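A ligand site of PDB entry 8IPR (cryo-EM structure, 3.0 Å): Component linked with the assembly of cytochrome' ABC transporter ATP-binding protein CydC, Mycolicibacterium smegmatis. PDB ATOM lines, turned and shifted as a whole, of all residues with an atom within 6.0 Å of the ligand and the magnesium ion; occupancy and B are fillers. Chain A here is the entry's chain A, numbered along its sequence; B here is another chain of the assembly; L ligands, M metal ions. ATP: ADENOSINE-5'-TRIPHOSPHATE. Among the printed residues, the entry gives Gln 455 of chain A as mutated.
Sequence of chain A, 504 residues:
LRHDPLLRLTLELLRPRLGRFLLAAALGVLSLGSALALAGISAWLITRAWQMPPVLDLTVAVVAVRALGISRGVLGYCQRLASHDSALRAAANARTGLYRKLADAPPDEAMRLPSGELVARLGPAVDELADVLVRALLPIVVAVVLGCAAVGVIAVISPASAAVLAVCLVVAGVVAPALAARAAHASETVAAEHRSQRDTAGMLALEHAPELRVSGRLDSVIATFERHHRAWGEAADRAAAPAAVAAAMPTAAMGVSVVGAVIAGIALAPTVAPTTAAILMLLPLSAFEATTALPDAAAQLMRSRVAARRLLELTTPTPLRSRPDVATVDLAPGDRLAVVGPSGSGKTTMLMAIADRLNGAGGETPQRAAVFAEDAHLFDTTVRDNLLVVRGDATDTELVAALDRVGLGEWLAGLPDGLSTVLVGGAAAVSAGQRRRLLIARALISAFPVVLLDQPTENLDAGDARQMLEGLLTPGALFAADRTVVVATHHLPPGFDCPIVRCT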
ATOM      1  N   ASP A 108      36.989  -9.952  12.551  1.00  0.00           N
ATOM      2  CA  ASP A 108      35.655  -9.420  12.294  1.00  0.00           C
ATOM      3  C   ASP A 108      35.382  -9.211  10.810  1.00  0.00           C
ATOM      4  O   ASP A 108      34.211  -9.114  10.421  1.00  0.00           O
ATOM      5  CB  ASP A 108      35.461  -8.110  13.052  1.00  0.00           C
ATOM      6  CG  ASP A 108      35.212  -8.327  14.532  1.00  0.00           C
ATOM      7  OD1 ASP A 108      34.884  -9.462  14.927  1.00  0.00           O
ATOM      8  OD2 ASP A 108      35.339  -7.354  15.308  1.00  0.00           O
ATOM      9  N   LEU A 320      33.641  -2.144   9.916  1.00  0.00           N
ATOM     10  CA  LEU A 320      32.535  -1.665  10.734  1.00  0.00           C
ATOM     11  C   LEU A 320      33.048  -0.580  11.674  1.00  0.00           C
ATOM     12  O   LEU A 320      34.174  -0.082  11.543  1.00  0.00           O
ATOM     13  CB  LEU A 320      31.894  -2.818  11.494  1.00  0.00           C
ATOM     14  CG  LEU A 320      31.736  -4.160  10.786  1.00  0.00           C
ATOM     15  CD1 LEU A 320      31.495  -5.265  11.790  1.00  0.00           C
ATOM     16  CD2 LEU A 320      30.588  -4.086   9.785  1.00  0.00           C
ATOM     17  N   ARG A 321      32.225  -0.200  12.647  1.00  0.00           N
ATOM     18  CA  ARG A 321      32.645   0.762  13.648  1.00  0.00           C
ATOM     19  C   ARG A 321      33.720   0.154  14.555  1.00  0.00           C
ATOM     20  O   ARG A 321      33.929  -1.058  14.583  1.00  0.00           O
ATOM     21  CB  ARG A 321      31.445   1.234  14.481  1.00  0.00           C
ATOM     22  CG  ARG A 321      30.732   0.107  15.202  1.00  0.00           C
ATOM     23  CD  ARG A 321      29.613   0.638  16.083  1.00  0.00           C
ATOM     24  NE  ARG A 321      28.948  -0.436  16.821  1.00  0.00           N
ATOM     25  CZ  ARG A 321      27.907  -0.257  17.614  1.00  0.00           C
ATOM     26  NH1 ARG A 321      27.374   0.929  17.820  1.00  0.00           N
ATOM     27  NH2 ARG A 321      27.390  -1.315  18.238  1.00  0.00           N
ATOM     28  N   SER A 322      34.393   1.019  15.303  1.00  0.00           N
ATOM     29  CA  SER A 322      35.467   0.609  16.183  1.00  0.00           C
ATOM     30  C   SER A 322      34.970   0.500  17.620  1.00  0.00           C
ATOM     31  O   SER A 322      34.163   1.330  18.067  1.00  0.00           O
ATOM     32  CB  SER A 322      36.635   1.599  16.119  1.00  0.00           C
ATOM     33  OG  SER A 322      37.086   1.756  14.784  1.00  0.00           O
ATOM     34  N   ARG A 323      35.445  -0.518  18.328  1.00  0.00           N
ATOM     35  CA  ARG A 323      35.067  -0.685  19.721  1.00  0.00           C
ATOM     36  C   ARG A 323      35.620   0.474  20.552  1.00  0.00           C
ATOM     37  O   ARG A 323      36.698   0.994  20.263  1.00  0.00           O
ATOM     38  CB  ARG A 323      35.596  -2.013  20.262  1.00  0.00           C
ATOM     39  CG  ARG A 323      35.441  -3.173  19.287  1.00  0.00           C
ATOM     40  CD  ARG A 323      35.835  -4.500  19.910  1.00  0.00           C
ATOM     41  NE  ARG A 323      34.811  -5.032  20.792  1.00  0.00           N
ATOM     42  CZ  ARG A 323      34.350  -6.276  20.747  1.00  0.00           C
ATOM     43  NH1 ARG A 323      34.791  -7.140  19.854  1.00  0.00           N
ATOM     44  NH2 ARG A 323      33.412  -6.657  21.604  1.00  0.00           N
ATOM     45  N   PRO A 324      34.892   0.913  21.584  1.00  0.00           N
ATOM     46  CA  PRO A 324      35.320   2.101  22.332  1.00  0.00           C
ATOM     47  C   PRO A 324      36.638   1.874  23.052  1.00  0.00           C
ATOM     48  O   PRO A 324      36.986   0.759  23.431  1.00  0.00           O
ATOM     49  CB  PRO A 324      34.174   2.328  23.334  1.00  0.00           C
ATOM     50  CG  PRO A 324      33.088   1.409  22.969  1.00  0.00           C
ATOM     51  CD  PRO A 324      33.611   0.370  22.034  1.00  0.00           C
ATOM     52  N   PRO A 342      27.792  -3.295  33.510  1.00  0.00           N
ATOM     53  CA  PRO A 342      26.522  -3.575  32.822  1.00  0.00           C
ATOM     54  C   PRO A 342      26.716  -4.349  31.525  1.00  0.00           C
ATOM     55  O   PRO A 342      27.837  -4.713  31.177  1.00  0.00           O
ATOM     56  CB  PRO A 342      25.948  -2.177  32.561  1.00  0.00           C
ATOM     57  CG  PRO A 342      27.108  -1.252  32.657  1.00  0.00           C
ATOM     58  CD  PRO A 342      28.047  -1.860  33.645  1.00  0.00           C
ATOM     59  N   SER A 343      25.623  -4.598  30.815  1.00  0.00           N
ATOM     60  CA  SER A 343      25.621  -5.473  29.649  1.00  0.00           C
ATOM     61  C   SER A 343      25.983  -4.752  28.352  1.00  0.00           C
ATOM     62  O   SER A 343      25.752  -5.290  27.266  1.00  0.00           O
ATOM     63  CB  SER A 343      24.266  -6.161  29.507  1.00  0.00           C
ATOM     64  OG  SER A 343      23.965  -6.422  28.145  1.00  0.00           O
ATOM     65  N   GLY A 344      26.521  -3.542  28.437  1.00  0.00           N
ATOM     66  CA  GLY A 344      26.991  -2.842  27.261  1.00  0.00           C
ATOM     67  C   GLY A 344      28.225  -2.006  27.527  1.00  0.00           C
ATOM     68  O   GLY A 344      28.609  -1.178  26.702  1.00  0.00           O
ATOM     69  N   SER A 345      28.861  -2.243  28.676  1.00  0.00           N
ATOM     70  CA  SER A 345      29.919  -1.366  29.136  1.00  0.00           C
ATOM     71  C   SER A 345      31.231  -1.568  28.395  1.00  0.00           C
ATOM     72  O   SER A 345      31.954  -0.598  28.151  1.00  0.00           O
ATOM     73  CB  SER A 345      30.128  -1.556  30.643  1.00  0.00           C
ATOM     74  OG  SER A 345      30.220  -2.930  30.969  1.00  0.00           O
ATOM     75  N   GLY A 346      31.572  -2.805  28.031  1.00  0.00           N
ATOM     76  CA  GLY A 346      32.820  -3.036  27.330  1.00  0.00           C
ATOM     77  C   GLY A 346      33.811  -3.923  28.047  1.00  0.00           C
ATOM     78  O   GLY A 346      35.028  -3.708  27.941  1.00  0.00           O
ATOM     79  N   LYS A 347      33.321  -4.912  28.795  1.00  0.00           N
ATOM     80  CA  LYS A 347      34.217  -5.840  29.480  1.00  0.00           C
ATOM     81  C   LYS A 347      35.021  -6.674  28.487  1.00  0.00           C
ATOM     82  O   LYS A 347      36.230  -6.880  28.680  1.00  0.00           O
ATOM     83  CB  LYS A 347      33.414  -6.742  30.407  1.00  0.00           C
ATOM     84  CG  LYS A 347      32.516  -6.000  31.366  1.00  0.00           C
ATOM     85  CD  LYS A 347      31.706  -6.945  32.228  1.00  0.00           C
ATOM     86  CE  LYS A 347      30.716  -7.713  31.393  1.00  0.00           C
ATOM     87  NZ  LYS A 347      29.393  -7.037  31.380  1.00  0.00           N
ATOM     88  N   THR A 348      34.377  -7.180  27.428  1.00  0.00           N
ATOM     89  CA  THR A 348      35.109  -7.921  26.407  1.00  0.00           C
ATOM     90  C   THR A 348      36.119  -7.034  25.699  1.00  0.00           C
ATOM     91  O   THR A 348      37.223  -7.472  25.370  1.00  0.00           O
ATOM     92  CB  THR A 348      34.126  -8.525  25.399  1.00  0.00           C
ATOM     93  OG1 THR A 348      33.073  -9.192  26.094  1.00  0.00           O
ATOM     94  CG2 THR A 348      34.849  -9.528  24.514  1.00  0.00           C
ATOM     95  N   THR A 349      35.743  -5.778  25.440  1.00  0.00           N
ATOM     96  CA  THR A 349      36.673  -4.831  24.840  1.00  0.00           C
ATOM     97  C   THR A 349      37.889  -4.620  25.726  1.00  0.00           C
ATOM     98  O   THR A 349      39.024  -4.579  25.233  1.00  0.00           O
ATOM     99  CB  THR A 349      35.969  -3.510  24.570  1.00  0.00           C
ATOM    100  OG1 THR A 349      34.732  -3.750  23.889  1.00  0.00           O
ATOM    101  CG2 THR A 349      36.845  -2.602  23.718  1.00  0.00           C
ATOM    102  N   MET A 350      37.681  -4.503  27.041  1.00  0.00           N
ATOM    103  CA  MET A 350      38.812  -4.328  27.946  1.00  0.00           C
ATOM    104  C   MET A 350      39.664  -5.588  28.005  1.00  0.00           C
ATOM    105  O   MET A 350      40.891  -5.493  28.098  1.00  0.00           O
ATOM    106  CB  MET A 350      38.319  -3.933  29.334  1.00  0.00           C
ATOM    107  CG  MET A 350      39.447  -3.766  30.341  1.00  0.00           C
ATOM    108  SD  MET A 350      38.941  -3.064  31.920  1.00  0.00           S
ATOM    109  CE  MET A 350      37.369  -2.329  31.477  1.00  0.00           C
ATOM    110  N   ASP A 454      35.973 -14.904  29.282  1.00  0.00           N
ATOM    111  CA  ASP A 454      34.833 -14.035  29.003  1.00  0.00           C
ATOM    112  C   ASP A 454      33.556 -14.787  29.350  1.00  0.00           C
ATOM    113  O   ASP A 454      33.129 -15.678  28.612  1.00  0.00           O
ATOM    114  CB  ASP A 454      34.842 -13.619  27.530  1.00  0.00           C
ATOM    115  CG  ASP A 454      34.232 -12.252  27.321  1.00  0.00           C
ATOM    116  OD1 ASP A 454      34.586 -11.314  28.068  1.00  0.00           O
ATOM    117  OD2 ASP A 454      33.400 -12.112  26.394  1.00  0.00           O
ATOM    118  N   GLN A 455      32.941 -14.408  30.479  1.00  0.00           N
ATOM    119  CA  GLN A 455      31.712 -15.018  30.973  1.00  0.00           C
ATOM    120  C   GLN A 455      31.833 -16.543  30.987  1.00  0.00           C
ATOM    121  O   GLN A 455      31.124 -17.231  30.242  1.00  0.00           O
ATOM    122  CB  GLN A 455      30.515 -14.593  30.133  1.00  0.00           C
ATOM    123  CG  GLN A 455      29.812 -13.353  30.643  1.00  0.00           C
ATOM    124  CD  GLN A 455      29.292 -12.458  29.534  1.00  0.00           C
ATOM    125  OE1 GLN A 455      28.188 -12.650  29.037  1.00  0.00           O
ATOM    126  NE2 GLN A 455      30.094 -11.483  29.133  1.00  0.00           N
ATOM    127  N   HIS A 490      29.225 -11.727  35.054  1.00  0.00           N
ATOM    128  CA  HIS A 490      28.002 -11.064  35.445  1.00  0.00           C
ATOM    129  C   HIS A 490      27.421 -11.580  36.759  1.00  0.00           C
ATOM    130  O   HIS A 490      26.443 -11.002  37.249  1.00  0.00           O
ATOM    131  CB  HIS A 490      26.933 -11.214  34.348  1.00  0.00           C
ATOM    132  CG  HIS A 490      26.924 -10.110  33.347  1.00  0.00           C
ATOM    133  ND1 HIS A 490      26.673  -8.794  33.696  1.00  0.00           N
ATOM    134  CD2 HIS A 490      27.118 -10.111  32.015  1.00  0.00           C
ATOM    135  CE1 HIS A 490      26.727  -8.039  32.616  1.00  0.00           C
ATOM    136  NE2 HIS A 490      26.991  -8.810  31.586  1.00  0.00           N
ATOM    137  N   GLU B 421      22.191   3.886  21.404  1.00  0.00           N
ATOM    138  CA  GLU B 421      23.641   4.019  21.467  1.00  0.00           C
ATOM    139  C   GLU B 421      24.321   3.679  20.145  1.00  0.00           C
ATOM    140  O   GLU B 421      25.480   4.048  19.943  1.00  0.00           O
ATOM    141  CB  GLU B 421      24.214   3.153  22.576  1.00  0.00           C
ATOM    142  CG  GLU B 421      24.292   1.669  22.248  1.00  0.00           C
ATOM    143  CD  GLU B 421      24.801   0.840  23.409  1.00  0.00           C
ATOM    144  OE1 GLU B 421      25.239   1.434  24.420  1.00  0.00           O
ATOM    145  OE2 GLU B 421      24.766  -0.403  23.323  1.00  0.00           O
ATOM    146  N   LEU B 422      23.633   2.989  19.240  1.00  0.00           N
ATOM    147  CA  LEU B 422      24.194   2.723  17.919  1.00  0.00           C
ATOM    148  C   LEU B 422      24.155   3.988  17.076  1.00  0.00           C
ATOM    149  O   LEU B 422      23.107   4.632  16.986  1.00  0.00           O
ATOM    150  CB  LEU B 422      23.427   1.603  17.219  1.00  0.00           C
ATOM    151  CG  LEU B 422      23.424   0.236  17.891  1.00  0.00           C
ATOM    152  CD1 LEU B 422      22.503  -0.718  17.148  1.00  0.00           C
ATOM    153  CD2 LEU B 422      24.819  -0.335  17.965  1.00  0.00           C
ATOM    154  N   GLY B 434      25.909 -12.310  14.628  1.00  0.00           N
ATOM    155  CA  GLY B 434      25.696 -11.153  15.467  1.00  0.00           C
ATOM    156  C   GLY B 434      26.906 -10.287  15.716  1.00  0.00           C
ATOM    157  O   GLY B 434      26.853  -9.420  16.596  1.00  0.00           O
ATOM    158  N   VAL B 435      27.996 -10.496  14.971  1.00  0.00           N
ATOM    159  CA  VAL B 435      29.189  -9.659  15.143  1.00  0.00           C
ATOM    160  C   VAL B 435      28.839  -8.209  14.859  1.00  0.00           C
ATOM    161  O   VAL B 435      28.148  -7.893  13.878  1.00  0.00           O
ATOM    162  CB  VAL B 435      30.315 -10.153  14.226  1.00  0.00           C
ATOM    163  CG1 VAL B 435      31.552  -9.293  14.408  1.00  0.00           C
ATOM    164  CG2 VAL B 435      30.642 -11.606  14.528  1.00  0.00           C
ATOM    165  N   GLY B 436      29.320  -7.316  15.722  1.00  0.00           N
ATOM    166  CA  GLY B 436      28.876  -5.943  15.747  1.00  0.00           C
ATOM    167  C   GLY B 436      27.945  -5.612  16.891  1.00  0.00           C
ATOM    168  O   GLY B 436      27.693  -4.430  17.147  1.00  0.00           O
ATOM    169  N   LEU B 437      27.436  -6.629  17.571  1.00  0.00           N
ATOM    170  CA  LEU B 437      26.636  -6.466  18.777  1.00  0.00           C
ATOM    171  C   LEU B 437      27.233  -7.331  19.868  1.00  0.00           C
ATOM    172  O   LEU B 437      27.856  -8.357  19.596  1.00  0.00           O
ATOM    173  CB  LEU B 437      25.162  -6.855  18.545  1.00  0.00           C
ATOM    174  CG  LEU B 437      24.215  -5.842  17.906  1.00  0.00           C
ATOM    175  CD1 LEU B 437      22.774  -6.268  18.147  1.00  0.00           C
ATOM    176  CD2 LEU B 437      24.453  -4.448  18.430  1.00  0.00           C
ATOM    177  N   SER B 438      27.048  -6.917  21.114  1.00  0.00           N
ATOM    178  CA  SER B 438      27.523  -7.703  22.236  1.00  0.00           C
ATOM    179  C   SER B 438      26.533  -8.815  22.551  1.00  0.00           C
ATOM    180  O   SER B 438      25.427  -8.875  22.016  1.00  0.00           O
ATOM    181  CB  SER B 438      27.756  -6.832  23.458  1.00  0.00           C
ATOM    182  OG  SER B 438      26.544  -6.407  24.024  1.00  0.00           O
ATOM    183  N   LEU B 439      26.941  -9.722  23.442  1.00  0.00           N
ATOM    184  CA  LEU B 439      26.124 -10.896  23.737  1.00  0.00           C
ATOM    185  C   LEU B 439      24.824 -10.514  24.434  1.00  0.00           C
ATOM    186  O   LEU B 439      23.771 -11.109  24.158  1.00  0.00           O
ATOM    187  CB  LEU B 439      26.920 -11.884  24.575  1.00  0.00           C
ATOM    188  CG  LEU B 439      28.020 -12.570  23.764  1.00  0.00           C
ATOM    189  CD1 LEU B 439      29.186 -12.984  24.651  1.00  0.00           C
ATOM    190  CD2 LEU B 439      27.453 -13.741  22.994  1.00  0.00           C
ATOM    191  N   GLY B 440      24.873  -9.549  25.347  1.00  0.00           N
ATOM    192  CA  GLY B 440      23.649  -9.072  25.966  1.00  0.00           C
ATOM    193  C   GLY B 440      22.718  -8.408  24.970  1.00  0.00           C
ATOM    194  O   GLY B 440      21.503  -8.579  25.030  1.00  0.00           O
ATOM    195  N   GLN B 441      23.288  -7.665  24.019  1.00  0.00           N
ATOM    196  CA  GLN B 441      22.471  -7.020  23.003  1.00  0.00           C
ATOM    197  C   GLN B 441      21.899  -8.030  22.019  1.00  0.00           C
ATOM    198  O   GLN B 441      20.754  -7.886  21.575  1.00  0.00           O
ATOM    199  CB  GLN B 441      23.304  -5.952  22.289  1.00  0.00           C
ATOM    200  CG  GLN B 441      23.885  -4.938  23.253  1.00  0.00           C
ATOM    201  CD  GLN B 441      24.729  -3.883  22.561  1.00  0.00           C
ATOM    202  OE1 GLN B 441      25.319  -4.125  21.522  1.00  0.00           O
ATOM    203  NE2 GLN B 441      24.791  -2.700  23.163  1.00  0.00           N
ATOM    204  N   ARG B 442      22.664  -9.064  21.677  1.00  0.00           N
ATOM    205  CA  ARG B 442      22.119 -10.150  20.857  1.00  0.00           C
ATOM    206  C   ARG B 442      20.980 -10.852  21.581  1.00  0.00           C
ATOM    207  O   ARG B 442      19.946 -11.189  20.978  1.00  0.00           O
ATOM    208  CB  ARG B 442      23.219 -11.145  20.503  1.00  0.00           C
ATOM    209  CG  ARG B 442      24.317 -10.594  19.624  1.00  0.00           C
ATOM    210  CD  ARG B 442      25.433 -11.619  19.447  1.00  0.00           C
ATOM    211  NE  ARG B 442      26.747 -11.026  19.590  1.00  0.00           N
ATOM    212  CZ  ARG B 442      27.885 -11.640  19.267  1.00  0.00           C
ATOM    213  NH1 ARG B 442      27.901 -12.868  18.789  1.00  0.00           N
ATOM    214  NH2 ARG B 442      29.041 -10.987  19.431  1.00  0.00           N
ATOM    215  N   ARG B 444      19.024  -9.540  23.845  1.00  0.00           N
ATOM    216  CA  ARG B 444      17.877  -8.648  23.856  1.00  0.00           C
ATOM    217  C   ARG B 444      17.198  -8.562  22.491  1.00  0.00           C
ATOM    218  O   ARG B 444      15.970  -8.423  22.427  1.00  0.00           O
ATOM    219  CB  ARG B 444      18.282  -7.262  24.332  1.00  0.00           C
ATOM    220  CG  ARG B 444      18.407  -7.159  25.844  1.00  0.00           C
ATOM    221  CD  ARG B 444      18.866  -5.780  26.265  1.00  0.00           C
ATOM    222  NE  ARG B 444      20.318  -5.670  26.270  1.00  0.00           N
ATOM    223  CZ  ARG B 444      20.981  -4.548  26.528  1.00  0.00           C
ATOM    224  NH1 ARG B 444      20.354  -3.418  26.815  1.00  0.00           N
ATOM    225  NH2 ARG B 444      22.312  -4.562  26.501  1.00  0.00           N
ATOM    226  N   HIS B 466      23.588 -13.567  29.762  1.00  0.00           N
ATOM    227  CA  HIS B 466      24.434 -12.432  29.413  1.00  0.00           C
ATOM    228  C   HIS B 466      23.846 -11.084  29.825  1.00  0.00           C
ATOM    229  O   HIS B 466      24.223 -10.053  29.286  1.00  0.00           O
ATOM    230  CB  HIS B 466      24.753 -12.408  27.915  1.00  0.00           C
ATOM    231  CG  HIS B 466      25.021 -13.757  27.318  1.00  0.00           C
ATOM    232  ND1 HIS B 466      24.069 -14.439  26.586  1.00  0.00           N
ATOM    233  CD2 HIS B 466      26.123 -14.540  27.330  1.00  0.00           C
ATOM    234  CE1 HIS B 466      24.573 -15.595  26.182  1.00  0.00           C
ATOM    235  NE2 HIS B 466      25.820 -15.676  26.614  1.00  0.00           N
HETATM  236  PG  ATP L   1      27.989  -8.084  27.338  1.00  0.00           P
HETATM  237  O1G ATP L   1      26.651  -7.857  26.768  1.00  0.00           O
HETATM  238  O2G ATP L   1      27.923  -8.361  28.767  1.00  0.00           O
HETATM  239  O3G ATP L   1      28.757  -9.089  26.598  1.00  0.00           O
HETATM  240  PB  ATP L   1      30.317  -6.276  27.213  1.00  0.00           P
HETATM  241  O1B ATP L   1      30.525  -5.456  28.401  1.00  0.00           O
HETATM  242  O2B ATP L   1      31.115  -7.478  26.988  1.00  0.00           O
HETATM  243  O3B ATP L   1      28.791  -6.718  27.177  1.00  0.00           O
HETATM  244  PA  ATP L   1      31.352  -5.375  24.603  1.00  0.00           P
HETATM  245  O1A ATP L   1      31.082  -6.620  23.854  1.00  0.00           O
HETATM  246  O2A ATP L   1      32.770  -4.996  24.812  1.00  0.00           O
HETATM  247  O3A ATP L   1      30.496  -5.347  25.936  1.00  0.00           O
HETATM  248  O5' ATP L   1      30.660  -4.190  23.837  1.00  0.00           O
HETATM  249  C5' ATP L   1      30.887  -2.823  24.202  1.00  0.00           C
HETATM  250  C4' ATP L   1      30.309  -1.983  23.106  1.00  0.00           C
HETATM  251  O4' ATP L   1      31.084  -2.212  21.917  1.00  0.00           O
HETATM  252  C3' ATP L   1      28.867  -2.338  22.720  1.00  0.00           C
HETATM  253  O3' ATP L   1      28.097  -1.177  22.477  1.00  0.00           O
HETATM  254  C2' ATP L   1      29.047  -3.110  21.422  1.00  0.00           C
HETATM  255  O2' ATP L   1      27.882  -3.070  20.647  1.00  0.00           O
HETATM  256  C1' ATP L   1      30.194  -2.298  20.845  1.00  0.00           C
HETATM  257  N9  ATP L   1      30.901  -2.782  19.665  1.00  0.00           N
HETATM  258  C8  ATP L   1      31.444  -1.987  18.694  1.00  0.00           C
HETATM  259  N7  ATP L   1      31.993  -2.667  17.723  1.00  0.00           N
HETATM  260  C5  ATP L   1      31.789  -3.982  18.080  1.00  0.00           C
HETATM  261  C6  ATP L   1      32.143  -5.183  17.449  1.00  0.00           C
HETATM  262  N6  ATP L   1      32.801  -5.239  16.299  1.00  0.00           N
HETATM  263  N1  ATP L   1      31.780  -6.328  18.066  1.00  0.00           N
HETATM  264  C2  ATP L   1      31.122  -6.255  19.234  1.00  0.00           C
HETATM  265  N3  ATP L   1      30.741  -5.182  19.911  1.00  0.00           N
HETATM  266  C4  ATP L   1      31.102  -4.068  19.268  1.00  0.00           C
HETATM  267 MG    MG M   1      31.141  -9.669  25.569  1.00  0.00          MG
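An oxygen (O2G) of the ligand sits at hydrogen-bond distance from a ring nitrogen (NE2) of His 490, at 3.0 Å. O of Ser 343 sits close to O1G of the ligand (2.8 Å). A nitrogen (N6) of the ligand is in hydrogen-bond range of the side-chain carboxylate of Asp 108. N of Gly 440 of chain B is in hydrogen-bond range of O1G of the ligand (2.8 Å). An oxygen (O2A) of the ligand is in hydrogen-bond range of the side-chain hydroxyl (OG1) of Thr 349 (2.5 Å). An oxygen (O2') of the ligand is in hydrogen-bond range of the guanidinium group (NH2) of Arg 321 (3.0 Å). An oxygen (O1B) of the ligand is in hydrogen-bond range of the backbone NH (N) of Lys 347 (2.9 Å). The side-chain hydroxyl (OG) of Ser 438 of chain B sits at hydrogen-bond distance from an oxygen (O1G) of the ligand, 3.1 Å away. The backbone NH of Gly 346 sits at hydrogen-bond distance from an oxygen (O1B) of the ligand (2.9 Å). An oxygen (O2B) of the ligand sits at hydrogen-bond distance from the backbone NH (N) of Thr 348 (3.3 Å). The backbone NH of Thr 349 is in hydrogen-bond range of an oxygen (O2A) of the ligand (3.1 Å). An oxygen (O1A) of the ligand is in salt-bridge range of the guanidinium group (NH2) of Arg 323, at 3.2 Å. An oxygen (O2') of the ligand lies within hydrogen-bond range of the side-chain amide oxygen (OE1) of Gln 441 of chain B (2.9 Å). O2G of the ligand lies within salt-bridge range of NZ of Lys 347. The side-chain hydroxyl (OG1) of Thr 348 sits close to an oxygen (O2B) of the ligand. OG of Ser 343 lies within hydrogen-bond range of O1G of the ligand, at 3.3 Å.
The backbone carbonyl oxygen (O) of Pro 342 lies within hydrogen-bond range of the side-chain amino group (NZ) of Lys 347 (2.8 Å). The guanidinium group of Arg 442 of chain B lies within hydrogen-bond range of the backbone carbonyl oxygen of Leu 437 of chain B (2.9 Å). The side-chain hydroxyl (OG1) of Thr 348 sits close to the side-chain carboxylate (OD2) of Asp 454 (3.0 Å). N of Ser 438 of chain B lies within hydrogen-bond range of OE1 of Gln 441 of chain B, at 3.3 Å. The side-chain hydroxyl (OG) of Ser 345 is in hydrogen-bond range of the backbone carbonyl oxygen (O) of Pro 342 (3.0 Å). OG1 of Thr 349 is in hydrogen-bond range of NE of Arg 323 (3.4 Å). A ring nitrogen (NE2) of His 490 lies within hydrogen-bond range of the side-chain amino group (NZ) of Lys 347, at 3.0 Å. The side-chain hydroxyl of Ser 343 sits at hydrogen-bond distance from the guanidinium group of Arg 444 of chain B (3.0 Å).
CD of Pro 324 touches O4' of the ligand, at 3.6 Å. O of Pro 342 touches O1B of the ligand, 3.9 Å away. O of Gly 344 touches C5' of the ligand (3.8 Å). OG of Ser 345 touches O1B of the ligand, 3.6 Å away. NE2 of Gln 455 touches O3G of the ligand, 3.7 Å away. Glu 421 of chain B touches the ligand (OE2 to O3', 3.5 Å). Gly 436 of chain B touches the ligand (N to N1, 3.5 Å). Leu 437 of chain B touches the ligand. Leu 439 of chain B touches the ligand (N to O3G, 3.7 Å). Hydrophobic or aromatic side chains that line the ligand: Pro 324, His 490 and Leu 439 of chain B. Of the 31 residues printed, 21 come within 4 Å of the ligand. The nearest printed residue that does not touch the ligand is His 466 of chain B (4.1 Å).
Merely in contact with the magnesium ion: Asp 454 (3.4 Å) and Leu 439 of chain B (3.96 Å). Of the 31 residues printed, 3 come within 4 Å of the magnesium ion.
OG1 of Thr 348 is bound to the magnesium ion (2.1 Å). The magnesium ion has one donor atom within binding distance. Slightly farther from the magnesium ion lies an oxygen (O2B) of the ligand (2.6 Å). Slightly farther from the magnesium ion lies an oxygen (O3G) of the ligand (2.7 Å).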
